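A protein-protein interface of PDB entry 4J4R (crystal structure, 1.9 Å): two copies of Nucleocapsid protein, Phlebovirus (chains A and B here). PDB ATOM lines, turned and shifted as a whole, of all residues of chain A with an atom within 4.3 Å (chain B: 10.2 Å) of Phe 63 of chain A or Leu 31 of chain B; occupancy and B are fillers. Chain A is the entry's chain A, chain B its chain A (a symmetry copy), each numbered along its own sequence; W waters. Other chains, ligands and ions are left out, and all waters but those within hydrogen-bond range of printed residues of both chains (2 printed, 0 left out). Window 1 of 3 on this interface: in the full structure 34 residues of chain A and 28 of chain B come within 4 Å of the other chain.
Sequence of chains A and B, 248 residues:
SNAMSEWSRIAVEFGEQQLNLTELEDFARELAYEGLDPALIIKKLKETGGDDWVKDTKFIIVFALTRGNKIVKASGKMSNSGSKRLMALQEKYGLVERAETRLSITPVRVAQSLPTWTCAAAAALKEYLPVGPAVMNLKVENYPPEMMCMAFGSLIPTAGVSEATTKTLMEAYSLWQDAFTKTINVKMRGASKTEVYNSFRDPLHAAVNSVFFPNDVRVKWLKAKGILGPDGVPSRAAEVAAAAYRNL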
ATOM      1  N   PHE A  59     -21.654 -17.191  18.431  1.00  0.00           N
ATOM      2  CA  PHE A  59     -20.847 -17.475  17.246  1.00  0.00           C
ATOM      3  C   PHE A  59     -21.208 -18.830  16.635  1.00  0.00           C
ATOM      4  O   PHE A  59     -21.358 -18.944  15.424  1.00  0.00           O
ATOM      5  CB  PHE A  59     -19.357 -17.455  17.599  1.00  0.00           C
ATOM      6  CG  PHE A  59     -18.442 -17.485  16.394  1.00  0.00           C
ATOM      7  CD1 PHE A  59     -18.071 -16.307  15.763  1.00  0.00           C
ATOM      8  CD2 PHE A  59     -17.945 -18.690  15.906  1.00  0.00           C
ATOM      9  CE1 PHE A  59     -17.222 -16.330  14.659  1.00  0.00           C
ATOM     10  CE2 PHE A  59     -17.098 -18.724  14.819  1.00  0.00           C
ATOM     11  CZ  PHE A  59     -16.735 -17.538  14.191  1.00  0.00           C
ATOM     12  N   ILE A  60     -21.340 -19.858  17.477  1.00  0.00           N
ATOM     13  CA  ILE A  60     -21.757 -21.181  17.016  1.00  0.00           C
ATOM     14  C   ILE A  60     -23.128 -21.106  16.339  1.00  0.00           C
ATOM     15  O   ILE A  60     -23.367 -21.767  15.320  1.00  0.00           O
ATOM     16  CB  ILE A  60     -21.805 -22.195  18.187  1.00  0.00           C
ATOM     17  CG1 ILE A  60     -20.395 -22.422  18.748  1.00  0.00           C
ATOM     18  CG2 ILE A  60     -22.449 -23.525  17.743  1.00  0.00           C
ATOM     19  CD1 ILE A  60     -20.369 -22.986  20.167  1.00  0.00           C
ATOM     20  N   ILE A  61     -24.028 -20.292  16.885  1.00  0.00           N
ATOM     21  CA  ILE A  61     -25.373 -20.197  16.307  1.00  0.00           C
ATOM     22  C   ILE A  61     -25.362 -19.513  14.932  1.00  0.00           C
ATOM     23  O   ILE A  61     -26.075 -19.939  14.009  1.00  0.00           O
ATOM     24  CB  ILE A  61     -26.383 -19.538  17.290  1.00  0.00           C
ATOM     25  CG1 ILE A  61     -26.684 -20.510  18.432  1.00  0.00           C
ATOM     26  CG2 ILE A  61     -27.700 -19.219  16.580  1.00  0.00           C
ATOM     27  CD1 ILE A  61     -27.509 -19.908  19.561  1.00  0.00           C
ATOM     28  N   VAL A  62     -24.547 -18.475  14.779  1.00  0.00           N
ATOM     29  CA  VAL A  62     -24.417 -17.823  13.472  1.00  0.00           C
ATOM     30  C   VAL A  62     -23.909 -18.825  12.433  1.00  0.00           C
ATOM     31  O   VAL A  62     -24.397 -18.867  11.303  1.00  0.00           O
ATOM     32  CB  VAL A  62     -23.519 -16.583  13.526  1.00  0.00           C
ATOM     33  CG1 VAL A  62     -23.269 -16.042  12.109  1.00  0.00           C
ATOM     34  CG2 VAL A  62     -24.170 -15.503  14.369  1.00  0.00           C
ATOM     35  N   PHE A  63     -22.942 -19.645  12.831  1.00  0.00           N
ATOM     36  CA  PHE A  63     -22.486 -20.727  11.970  1.00  0.00           C
ATOM     37  C   PHE A  63     -23.627 -21.682  11.599  1.00  0.00           C
ATOM     38  O   PHE A  63     -23.812 -22.007  10.427  1.00  0.00           O
ATOM     39  CB  PHE A  63     -21.335 -21.505  12.610  1.00  0.00           C
ATOM     40  CG  PHE A  63     -20.887 -22.675  11.787  1.00  0.00           C
ATOM     41  CD1 PHE A  63     -20.096 -22.485  10.674  1.00  0.00           C
ATOM     42  CD2 PHE A  63     -21.287 -23.967  12.113  1.00  0.00           C
ATOM     43  CE1 PHE A  63     -19.685 -23.572   9.890  1.00  0.00           C
ATOM     44  CE2 PHE A  63     -20.890 -25.049  11.331  1.00  0.00           C
ATOM     45  CZ  PHE A  63     -20.084 -24.842  10.219  1.00  0.00           C
ATOM     46  N   ALA A  64     -24.396 -22.121  12.590  1.00  0.00           N
ATOM     47  CA  ALA A  64     -25.508 -23.032  12.332  1.00  0.00           C
ATOM     48  C   ALA A  64     -26.522 -22.415  11.377  1.00  0.00           C
ATOM     49  O   ALA A  64     -27.061 -23.105  10.507  1.00  0.00           O
ATOM     50  CB  ALA A  64     -26.187 -23.424  13.634  1.00  0.00           C
ATOM     51  N   LEU A  65     -26.793 -21.122  11.562  1.00  0.00           N
ATOM     52  CA  LEU A  65     -27.809 -20.409  10.784  1.00  0.00           C
ATOM     53  C   LEU A  65     -27.392 -20.274   9.328  1.00  0.00           C
ATOM     54  O   LEU A  65     -28.218 -20.361   8.416  1.00  0.00           O
ATOM     55  CB  LEU A  65     -28.006 -18.999  11.353  1.00  0.00           C
ATOM     56  CG  LEU A  65     -28.929 -18.901  12.555  1.00  0.00           C
ATOM     57  CD1 LEU A  65     -29.017 -17.463  13.049  1.00  0.00           C
ATOM     58  CD2 LEU A  65     -30.301 -19.421  12.147  1.00  0.00           C
ATOM     59  N   THR A  66     -26.102 -20.043   9.111  1.00  0.00           N
ATOM     60  CA  THR A  66     -25.628 -19.706   7.771  1.00  0.00           C
ATOM     61  C   THR A  66     -24.938 -20.856   7.031  1.00  0.00           C
ATOM     62  O   THR A  66     -24.920 -20.875   5.806  1.00  0.00           O
ATOM     63  CB  THR A  66     -24.718 -18.466   7.791  1.00  0.00           C
ATOM     64  OG1 THR A  66     -23.539 -18.740   8.555  1.00  0.00           O
ATOM     65  CG2 THR A  66     -25.447 -17.277   8.407  1.00  0.00           C
ATOM     66  N   ARG A  67     -24.354 -21.796   7.767  1.00  0.00           N
ATOM     67  CA  ARG A  67     -23.599 -22.884   7.140  1.00  0.00           C
ATOM     68  C   ARG A  67     -24.085 -24.291   7.528  1.00  0.00           C
ATOM     69  O   ARG A  67     -23.720 -25.270   6.879  1.00  0.00           O
ATOM     70  CB  ARG A  67     -22.109 -22.774   7.484  1.00  0.00           C
ATOM     71  CG  ARG A  67     -21.443 -21.442   7.138  1.00  0.00           C
ATOM     72  CD  ARG A  67     -21.519 -21.125   5.644  1.00  0.00           C
ATOM     73  NE  ARG A  67     -20.750 -22.047   4.797  1.00  0.00           N
ATOM     74  CZ  ARG A  67     -19.458 -21.914   4.503  1.00  0.00           C
ATOM     75  NH1 ARG A  67     -18.752 -20.910   5.025  1.00  0.00           N
ATOM     76  NH2 ARG A  67     -18.863 -22.797   3.694  1.00  0.00           N
ATOM     77  N   GLY A  68     -24.877 -24.397   8.593  1.00  0.00           N
ATOM     78  CA  GLY A  68     -25.411 -25.686   9.017  1.00  0.00           C
ATOM     79  C   GLY A  68     -24.501 -26.432   9.985  1.00  0.00           C
ATOM     80  O   GLY A  68     -23.900 -25.822  10.880  1.00  0.00           O
ATOM     81  N   LYS A  70     -21.955 -28.815   8.997  1.00  0.00           N
ATOM     82  CA  LYS A  70     -20.740 -29.406   8.440  1.00  0.00           C
ATOM     83  C   LYS A  70     -19.490 -28.590   8.744  1.00  0.00           C
ATOM     84  O   LYS A  70     -18.975 -27.838   7.899  1.00  0.00           O
ATOM     85  CB  LYS A  70     -20.913 -29.696   6.952  1.00  0.00           C
ATOM     86  CG  LYS A  70     -22.023 -30.720   6.703  1.00  0.00           C
ATOM     87  CD  LYS A  70     -21.836 -31.478   5.392  1.00  0.00           C
ATOM     88  CE  LYS A  70     -23.185 -31.912   4.830  1.00  0.00           C
ATOM     89  NZ  LYS A  70     -24.039 -30.716   4.564  1.00  0.00           N
ATOM     90  N   ILE A  71     -18.995 -28.772   9.963  1.00  0.00           N
ATOM     91  CA  ILE A  71     -17.901 -27.964  10.494  1.00  0.00           C
ATOM     92  C   ILE A  71     -16.627 -28.021   9.632  1.00  0.00           C
ATOM     93  O   ILE A  71     -16.111 -26.984   9.213  1.00  0.00           O
ATOM     94  CB  ILE A  71     -17.613 -28.361  11.967  1.00  0.00           C
ATOM     95  CG1 ILE A  71     -18.833 -28.063  12.845  1.00  0.00           C
ATOM     96  CG2 ILE A  71     -16.420 -27.625  12.517  1.00  0.00           C
ATOM     97  CD1 ILE A  71     -18.699 -28.579  14.265  1.00  0.00           C
ATOM     98  N   ALA A  74     -17.195 -26.790   5.816  1.00  0.00           N
ATOM     99  CA  ALA A  74     -17.423 -25.342   5.795  1.00  0.00           C
ATOM    100  C   ALA A  74     -16.173 -24.557   6.154  1.00  0.00           C
ATOM    101  O   ALA A  74     -15.890 -23.532   5.536  1.00  0.00           O
ATOM    102  CB  ALA A  74     -18.590 -24.949   6.706  1.00  0.00           C
ATOM    103  N   MET A  78     -14.059 -20.686   4.043  1.00  0.00           N
ATOM    104  CA  MET A  78     -14.457 -19.502   4.798  1.00  0.00           C
ATOM    105  C   MET A  78     -13.206 -18.722   5.140  1.00  0.00           C
ATOM    106  O   MET A  78     -12.086 -19.172   4.862  1.00  0.00           O
ATOM    107  CB  MET A  78     -15.267 -19.837   6.072  1.00  0.00           C
ATOM    108  CG  MET A  78     -14.501 -20.561   7.169  1.00  0.00           C
ATOM    109  SD  MET A  78     -15.386 -20.674   8.764  1.00  0.00           S
ATOM    110  CE  MET A  78     -16.908 -21.514   8.308  1.00  0.00           C
ATOM    111  N   GLY A  82     -12.652 -16.837  10.643  1.00  0.00           N
ATOM    112  CA  GLY A  82     -13.803 -17.679  10.926  1.00  0.00           C
ATOM    113  C   GLY A  82     -13.421 -19.125  11.160  1.00  0.00           C
ATOM    114  O   GLY A  82     -13.900 -19.768  12.099  1.00  0.00           O
ATOM    115  N   LEU A  86     -13.811 -21.176  14.647  1.00  0.00           N
ATOM    116  CA  LEU A  86     -14.710 -22.335  14.649  1.00  0.00           C
ATOM    117  C   LEU A  86     -13.998 -23.604  15.114  1.00  0.00           C
ATOM    118  O   LEU A  86     -14.533 -24.363  15.925  1.00  0.00           O
ATOM    119  CB  LEU A  86     -15.319 -22.546  13.260  1.00  0.00           C
ATOM    120  CG  LEU A  86     -16.301 -23.705  13.101  1.00  0.00           C
ATOM    121  CD1 LEU A  86     -17.570 -23.423  13.860  1.00  0.00           C
ATOM    122  CD2 LEU A  86     -16.612 -23.946  11.625  1.00  0.00           C
ATOM    123  N   PRO A 107     -23.827 -27.831  15.984  1.00  0.00           N
ATOM    124  CA  PRO A 107     -24.207 -26.414  15.895  1.00  0.00           C
ATOM    125  C   PRO A 107     -25.732 -26.202  15.804  1.00  0.00           C
ATOM    126  O   PRO A 107     -26.248 -25.268  16.419  1.00  0.00           O
ATOM    127  CB  PRO A 107     -23.498 -25.956  14.619  1.00  0.00           C
ATOM    128  CG  PRO A 107     -22.220 -26.772  14.635  1.00  0.00           C
ATOM    129  CD  PRO A 107     -22.685 -28.153  15.103  1.00  0.00           C
ATOM    130  N   GLU B  23     -21.671  -6.724  15.668  1.00  0.00           N
ATOM    131  CA  GLU B  23     -20.956  -7.936  16.035  1.00  0.00           C
ATOM    132  C   GLU B  23     -21.505  -9.153  15.274  1.00  0.00           C
ATOM    133  O   GLU B  23     -20.740  -9.962  14.750  1.00  0.00           O
ATOM    134  CB  GLU B  23     -21.051  -8.143  17.547  1.00  0.00           C
ATOM    135  CG  GLU B  23     -20.574  -9.495  18.038  1.00  0.00           C
ATOM    136  CD  GLU B  23     -20.582  -9.590  19.563  1.00  0.00           C
ATOM    137  OE1 GLU B  23     -21.632  -9.932  20.154  1.00  0.00           O
ATOM    138  OE2 GLU B  23     -19.528  -9.323  20.166  1.00  0.00           O
ATOM    139  N   LEU B  24     -22.827  -9.263  15.180  1.00  0.00           N
ATOM    140  CA  LEU B  24     -23.441 -10.367  14.430  1.00  0.00           C
ATOM    141  C   LEU B  24     -23.082 -10.357  12.938  1.00  0.00           C
ATOM    142  O   LEU B  24     -22.851 -11.414  12.352  1.00  0.00           O
ATOM    143  CB  LEU B  24     -24.963 -10.391  14.628  1.00  0.00           C
ATOM    144  CG  LEU B  24     -25.456 -10.870  15.994  1.00  0.00           C
ATOM    145  CD1 LEU B  24     -26.972 -11.016  15.995  1.00  0.00           C
ATOM    146  CD2 LEU B  24     -24.786 -12.190  16.373  1.00  0.00           C
ATOM    147  N   GLU B  25     -23.029  -9.180  12.315  1.00  0.00           N
ATOM    148  CA  GLU B  25     -22.611  -9.116  10.915  1.00  0.00           C
ATOM    149  C   GLU B  25     -21.130  -9.449  10.728  1.00  0.00           C
ATOM    150  O   GLU B  25     -20.759 -10.046   9.713  1.00  0.00           O
ATOM    151  CB  GLU B  25     -22.924  -7.751  10.293  1.00  0.00           C
ATOM    152  CG  GLU B  25     -24.405  -7.420  10.190  1.00  0.00           C
ATOM    153  CD  GLU B  25     -24.637  -5.980   9.734  1.00  0.00           C
ATOM    154  OE1 GLU B  25     -23.752  -5.121   9.967  1.00  0.00           O
ATOM    155  OE2 GLU B  25     -25.702  -5.711   9.132  1.00  0.00           O
ATOM    156  N   ASP B  26     -20.287  -9.055  11.679  1.00  0.00           N
ATOM    157  CA  ASP B  26     -18.875  -9.472  11.675  1.00  0.00           C
ATOM    158  C   ASP B  26     -18.800 -10.993  11.675  1.00  0.00           C
ATOM    159  O   ASP B  26     -18.090 -11.583  10.850  1.00  0.00           O
ATOM    160  CB  ASP B  26     -18.088  -8.929  12.886  1.00  0.00           C
ATOM    161  CG  ASP B  26     -16.603  -9.359  12.876  1.00  0.00           C
ATOM    162  OD1 ASP B  26     -15.914  -9.077  11.880  1.00  0.00           O
ATOM    163  OD2 ASP B  26     -16.101  -9.989  13.848  1.00  0.00           O
ATOM    164  N   PHE B  27     -19.517 -11.631  12.603  1.00  0.00           N
ATOM    165  CA  PHE B  27     -19.479 -13.093  12.702  1.00  0.00           C
ATOM    166  C   PHE B  27     -19.944 -13.720  11.395  1.00  0.00           C
ATOM    167  O   PHE B  27     -19.339 -14.668  10.897  1.00  0.00           O
ATOM    168  CB  PHE B  27     -20.384 -13.606  13.835  1.00  0.00           C
ATOM    169  CG  PHE B  27     -19.897 -13.266  15.222  1.00  0.00           C
ATOM    170  CD1 PHE B  27     -18.664 -12.657  15.417  1.00  0.00           C
ATOM    171  CD2 PHE B  27     -20.670 -13.585  16.333  1.00  0.00           C
ATOM    172  CE1 PHE B  27     -18.209 -12.349  16.708  1.00  0.00           C
ATOM    173  CE2 PHE B  27     -20.219 -13.291  17.628  1.00  0.00           C
ATOM    174  CZ  PHE B  27     -18.989 -12.669  17.806  1.00  0.00           C
ATOM    175  N   ALA B  28     -21.045 -13.205  10.858  1.00  0.00           N
ATOM    176  CA  ALA B  28     -21.640 -13.795   9.656  1.00  0.00           C
ATOM    177  C   ALA B  28     -20.714 -13.662   8.450  1.00  0.00           C
ATOM    178  O   ALA B  28     -20.654 -14.551   7.601  1.00  0.00           O
ATOM    179  CB  ALA B  28     -22.989 -13.167   9.367  1.00  0.00           C
ATOM    180  N   ARG B  29     -19.979 -12.558   8.373  1.00  0.00           N
ATOM    181  CA  ARG B  29     -19.000 -12.405   7.294  1.00  0.00           C
ATOM    182  C   ARG B  29     -17.798 -13.351   7.458  1.00  0.00           C
ATOM    183  O   ARG B  29     -17.311 -13.935   6.479  1.00  0.00           O
ATOM    184  CB  ARG B  29     -18.568 -10.935   7.171  1.00  0.00           C
ATOM    185  CG  ARG B  29     -19.617 -10.082   6.435  1.00  0.00           C
ATOM    186  CD  ARG B  29     -19.093  -8.709   6.059  1.00  0.00           C
ATOM    187  NE  ARG B  29     -19.329  -7.749   7.126  1.00  0.00           N
ATOM    188  CZ  ARG B  29     -20.323  -6.867   7.131  1.00  0.00           C
ATOM    189  NH1 ARG B  29     -21.168  -6.801   6.103  1.00  0.00           N
ATOM    190  NH2 ARG B  29     -20.457  -6.042   8.158  1.00  0.00           N
ATOM    191  N   GLU B  30     -17.323 -13.512   8.693  1.00  0.00           N
ATOM    192  CA  GLU B  30     -16.218 -14.447   8.971  1.00  0.00           C
ATOM    193  C   GLU B  30     -16.563 -15.910   8.672  1.00  0.00           C
ATOM    194  O   GLU B  30     -15.688 -16.707   8.301  1.00  0.00           O
ATOM    195  CB  GLU B  30     -15.745 -14.300  10.426  1.00  0.00           C
ATOM    196  CG  GLU B  30     -15.065 -12.975  10.672  1.00  0.00           C
ATOM    197  CD  GLU B  30     -14.814 -12.685  12.138  1.00  0.00           C
ATOM    198  OE1 GLU B  30     -15.615 -13.098  13.014  1.00  0.00           O
ATOM    199  OE2 GLU B  30     -13.794 -12.029  12.411  1.00  0.00           O
ATOM    200  N   LEU B  31     -17.840 -16.255   8.824  1.00  0.00           N
ATOM    201  CA  LEU B  31     -18.305 -17.636   8.655  1.00  0.00           C
ATOM    202  C   LEU B  31     -18.892 -17.932   7.280  1.00  0.00           C
ATOM    203  O   LEU B  31     -19.174 -19.088   6.958  1.00  0.00           O
ATOM    204  CB  LEU B  31     -19.356 -17.960   9.725  1.00  0.00           C
ATOM    205  CG  LEU B  31     -18.776 -18.026  11.131  1.00  0.00           C
ATOM    206  CD1 LEU B  31     -19.885 -17.942  12.185  1.00  0.00           C
ATOM    207  CD2 LEU B  31     -17.972 -19.327  11.267  1.00  0.00           C
ATOM    208  N   ALA B  32     -19.086 -16.883   6.477  1.00  0.00           N
ATOM    209  CA  ALA B  32     -19.697 -17.022   5.156  1.00  0.00           C
ATOM    210  C   ALA B  32     -18.802 -17.812   4.213  1.00  0.00           C
ATOM    211  O   ALA B  32     -17.578 -17.878   4.403  1.00  0.00           O
ATOM    212  CB  ALA B  32     -19.972 -15.669   4.564  1.00  0.00           C
ATOM    213  N   TYR B  33     -19.414 -18.388   3.183  1.00  0.00           N
ATOM    214  CA  TYR B  33     -18.651 -19.037   2.116  1.00  0.00           C
ATOM    215  C   TYR B  33     -17.537 -18.140   1.571  1.00  0.00           C
ATOM    216  O   TYR B  33     -17.761 -16.970   1.237  1.00  0.00           O
ATOM    217  CB  TYR B  33     -19.565 -19.455   0.968  1.00  0.00           C
ATOM    218  CG  TYR B  33     -18.863 -20.361  -0.024  1.00  0.00           C
ATOM    219  CD1 TYR B  33     -18.905 -21.744   0.124  1.00  0.00           C
ATOM    220  CD2 TYR B  33     -18.154 -19.832  -1.104  1.00  0.00           C
ATOM    221  CE1 TYR B  33     -18.269 -22.584  -0.779  1.00  0.00           C
ATOM    222  CE2 TYR B  33     -17.504 -20.664  -2.009  1.00  0.00           C
ATOM    223  CZ  TYR B  33     -17.574 -22.039  -1.842  1.00  0.00           C
ATOM    224  OH  TYR B  33     -16.943 -22.880  -2.729  1.00  0.00           O
ATOM    225  N   GLU B  34     -16.325 -18.687   1.515  1.00  0.00           N
ATOM    226  CA  GLU B  34     -15.223 -18.050   0.797  1.00  0.00           C
ATOM    227  C   GLU B  34     -14.582 -19.083  -0.128  1.00  0.00           C
ATOM    228  O   GLU B  34     -14.205 -20.168   0.330  1.00  0.00           O
ATOM    229  CB  GLU B  34     -14.178 -17.512   1.777  1.00  0.00           C
ATOM    230  CG  GLU B  34     -12.943 -16.914   1.095  1.00  0.00           C
ATOM    231  CD  GLU B  34     -11.921 -16.404   2.093  1.00  0.00           C
ATOM    232  OE1 GLU B  34     -10.759 -16.852   2.029  1.00  0.00           O
ATOM    233  OE2 GLU B  34     -12.278 -15.557   2.948  1.00  0.00           O
ATOM    234  N   GLY B  35     -14.443 -18.755  -1.413  1.00  0.00           N
ATOM    235  CA  GLY B  35     -13.919 -19.716  -2.383  1.00  0.00           C
ATOM    236  C   GLY B  35     -12.424 -19.588  -2.623  1.00  0.00           C
ATOM    237  O   GLY B  35     -11.744 -20.565  -2.977  1.00  0.00           O
ATOM    238  N   ARG B 102      -6.569 -23.429   0.807  1.00  0.00           N
ATOM    239  CA  ARG B 102      -6.398 -21.997   0.557  1.00  0.00           C
ATOM    240  C   ARG B 102      -5.194 -21.700  -0.316  1.00  0.00           C
ATOM    241  O   ARG B 102      -5.171 -20.700  -1.042  1.00  0.00           O
ATOM    242  CB  ARG B 102      -6.233 -21.255   1.885  1.00  0.00           C
ATOM    243  CG  ARG B 102      -7.418 -21.424   2.787  1.00  0.00           C
ATOM    244  CD  ARG B 102      -7.175 -20.913   4.201  1.00  0.00           C
ATOM    245  NE  ARG B 102      -8.282 -21.330   5.056  1.00  0.00           N
ATOM    246  CZ  ARG B 102      -9.453 -20.706   5.093  1.00  0.00           C
ATOM    247  NH1 ARG B 102      -9.645 -19.636   4.328  1.00  0.00           N
ATOM    248  NH2 ARG B 102     -10.425 -21.147   5.888  1.00  0.00           N
ATOM    249  N   ASP B 202     -23.229 -19.958  -3.825  1.00  0.00           N
ATOM    250  CA  ASP B 202     -22.265 -19.536  -2.808  1.00  0.00           C
ATOM    251  C   ASP B 202     -21.005 -18.884  -3.398  1.00  0.00           C
ATOM    252  O   ASP B 202     -20.607 -17.808  -2.939  1.00  0.00           O
ATOM    253  CB  ASP B 202     -21.899 -20.685  -1.850  1.00  0.00           C
ATOM    254  CG  ASP B 202     -23.060 -21.117  -0.982  1.00  0.00           C
ATOM    255  OD1 ASP B 202     -24.003 -20.320  -0.820  1.00  0.00           O
ATOM    256  OD2 ASP B 202     -23.024 -22.256  -0.465  1.00  0.00           O
ATOM    257  N   ALA B 206     -20.197 -14.957  -2.845  1.00  0.00           N
ATOM    258  CA  ALA B 206     -18.899 -14.647  -2.238  1.00  0.00           C
ATOM    259  C   ALA B 206     -18.093 -13.684  -3.110  1.00  0.00           C
ATOM    260  O   ALA B 206     -17.419 -12.785  -2.599  1.00  0.00           O
ATOM    261  CB  ALA B 206     -18.106 -15.915  -1.952  1.00  0.00           C
HETATM  262  O   HOH W   1     -11.253 -20.530   1.842  1.00  0.00           O
HETATM  263  O   HOH W   2     -22.171 -16.647   7.152  1.00  0.00           O
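Phe 27 of chain B touches Phe 59 of chain A. CE1 of Phe 59 of chain A touches OE1 of Glu 30 of chain B, at 3.97 Å. CD2 of Leu 24 of chain B touches CG2 of Val 62 of chain A, 3.9 Å away. CG1 of Val 62 of chain A touches CA of Ala 28 of chain B, at 3.7 Å. CG1 of Val 62 of chain A touches CD1 of Leu 31 of chain B (3.9 Å). N of Phe 63 of chain A touches CD1 of Leu 31 of chain B, 3.6 Å away. O of Glu 30 of chain B touches CB of Met 78 of chain A, 3.9 Å away. Leu 31 of chain B touches Met 78 of chain A (O to CE, 3.6 Å). Met 78 of chain A touches Glu 34 of chain B (CA to CB, 3.6 Å). Gly 82 of chain A touches Glu 30 of chain B.
No position is printed for both chains. Of the 16 pairs that touch across the chains among the printed residues, none has its exchanged pair printed and touching as well.
The guanidinium group (NH1) of Arg 67 of chain A is in hydrogen-bond range of the backbone carbonyl oxygen (O) of Leu 31 of chain B (2.7 Å). The guanidinium group (NH1) of Arg 67 of chain A sits close to the backbone carbonyl oxygen (O) of Ala 32 of chain B (3.3 Å). The backbone carbonyl oxygen (O) of Met 78 of chain A sits at hydrogen-bond distance from the guanidinium group (NH1) of Arg 102 of chain B (2.5 Å). NH1 of Arg 67 of chain A sits close to N of Tyr 33 of chain B, at 3.2 Å.
O of Val 62 of chain A is in hydrogen-bond range of OG1 of Thr 66 of chain A. The backbone NH (N) of Gly 68 of chain A sits at hydrogen-bond distance from the backbone carbonyl oxygen (O) of Phe 63 of chain A (3.2 Å). OE1 of Glu 34 of chain B is in salt-bridge range of NH1 of Arg 102 of chain B.
Along chain A the printed residues that touch a printed residue of chain B span positions 59 to 82. Printed residues of chain B that touch a printed residue of chain A: Leu 24, Phe 27, Ala 28, Glu 30, Leu 31, Ala 32, Tyr 33, Glu 34 and Arg 102.
Of the printed residues of chain B, Phe 63 of chain A touches Leu 31. Of the printed residues of chain A, Leu 31 of chain B touches Phe 59, Val 62, Phe 63, Arg 67 and Met 78. Val 62 of chain A touches just these residues of chain B: Leu 24, Ala 28 and Leu 31. No residue of chain B comes within 4 Å of Thr 66 of chain A. Of chain B, only Leu 31 (2.7 Å), Ala 32 (3.2 Å) and Tyr 33 (3.2 Å) come within 4 Å of Arg 67 of chain A. Gly 68 of chain A touches none of the printed residues of chain B. No residue of chain B comes within 4 Å of Ile 71 of chain A. Of the printed residues of chain A, Glu 34 of chain B touches Met 78. Of the printed residues of chain A, Arg 102 of chain B touches Met 78. The nearest residue of chain A that does not touch Leu 31 of chain B is Gly 82 of chain A (4.2 Å). The nearest printed residue of chain A that does not touch Ala 28 of chain B is Thr 66 of chain A (4.9 Å).
Water W2 lies within hydrogen-bond range of the backbone carbonyl oxygen (O) of Ala 28 of chain B, the side-chain hydroxyl (OG1) of Thr 66 of chain A and the backbone NH (N) of Ala 32 of chain B. Water W1 lies within hydrogen-bond range of the guanidinium group (NH1) of Arg 102 of chain B (3.1 Å), the backbone carbonyl oxygen (O) of Glu 34 of chain B (3.3 Å) and the backbone carbonyl oxygen (O) of Met 78 of chain A (3.4 Å).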
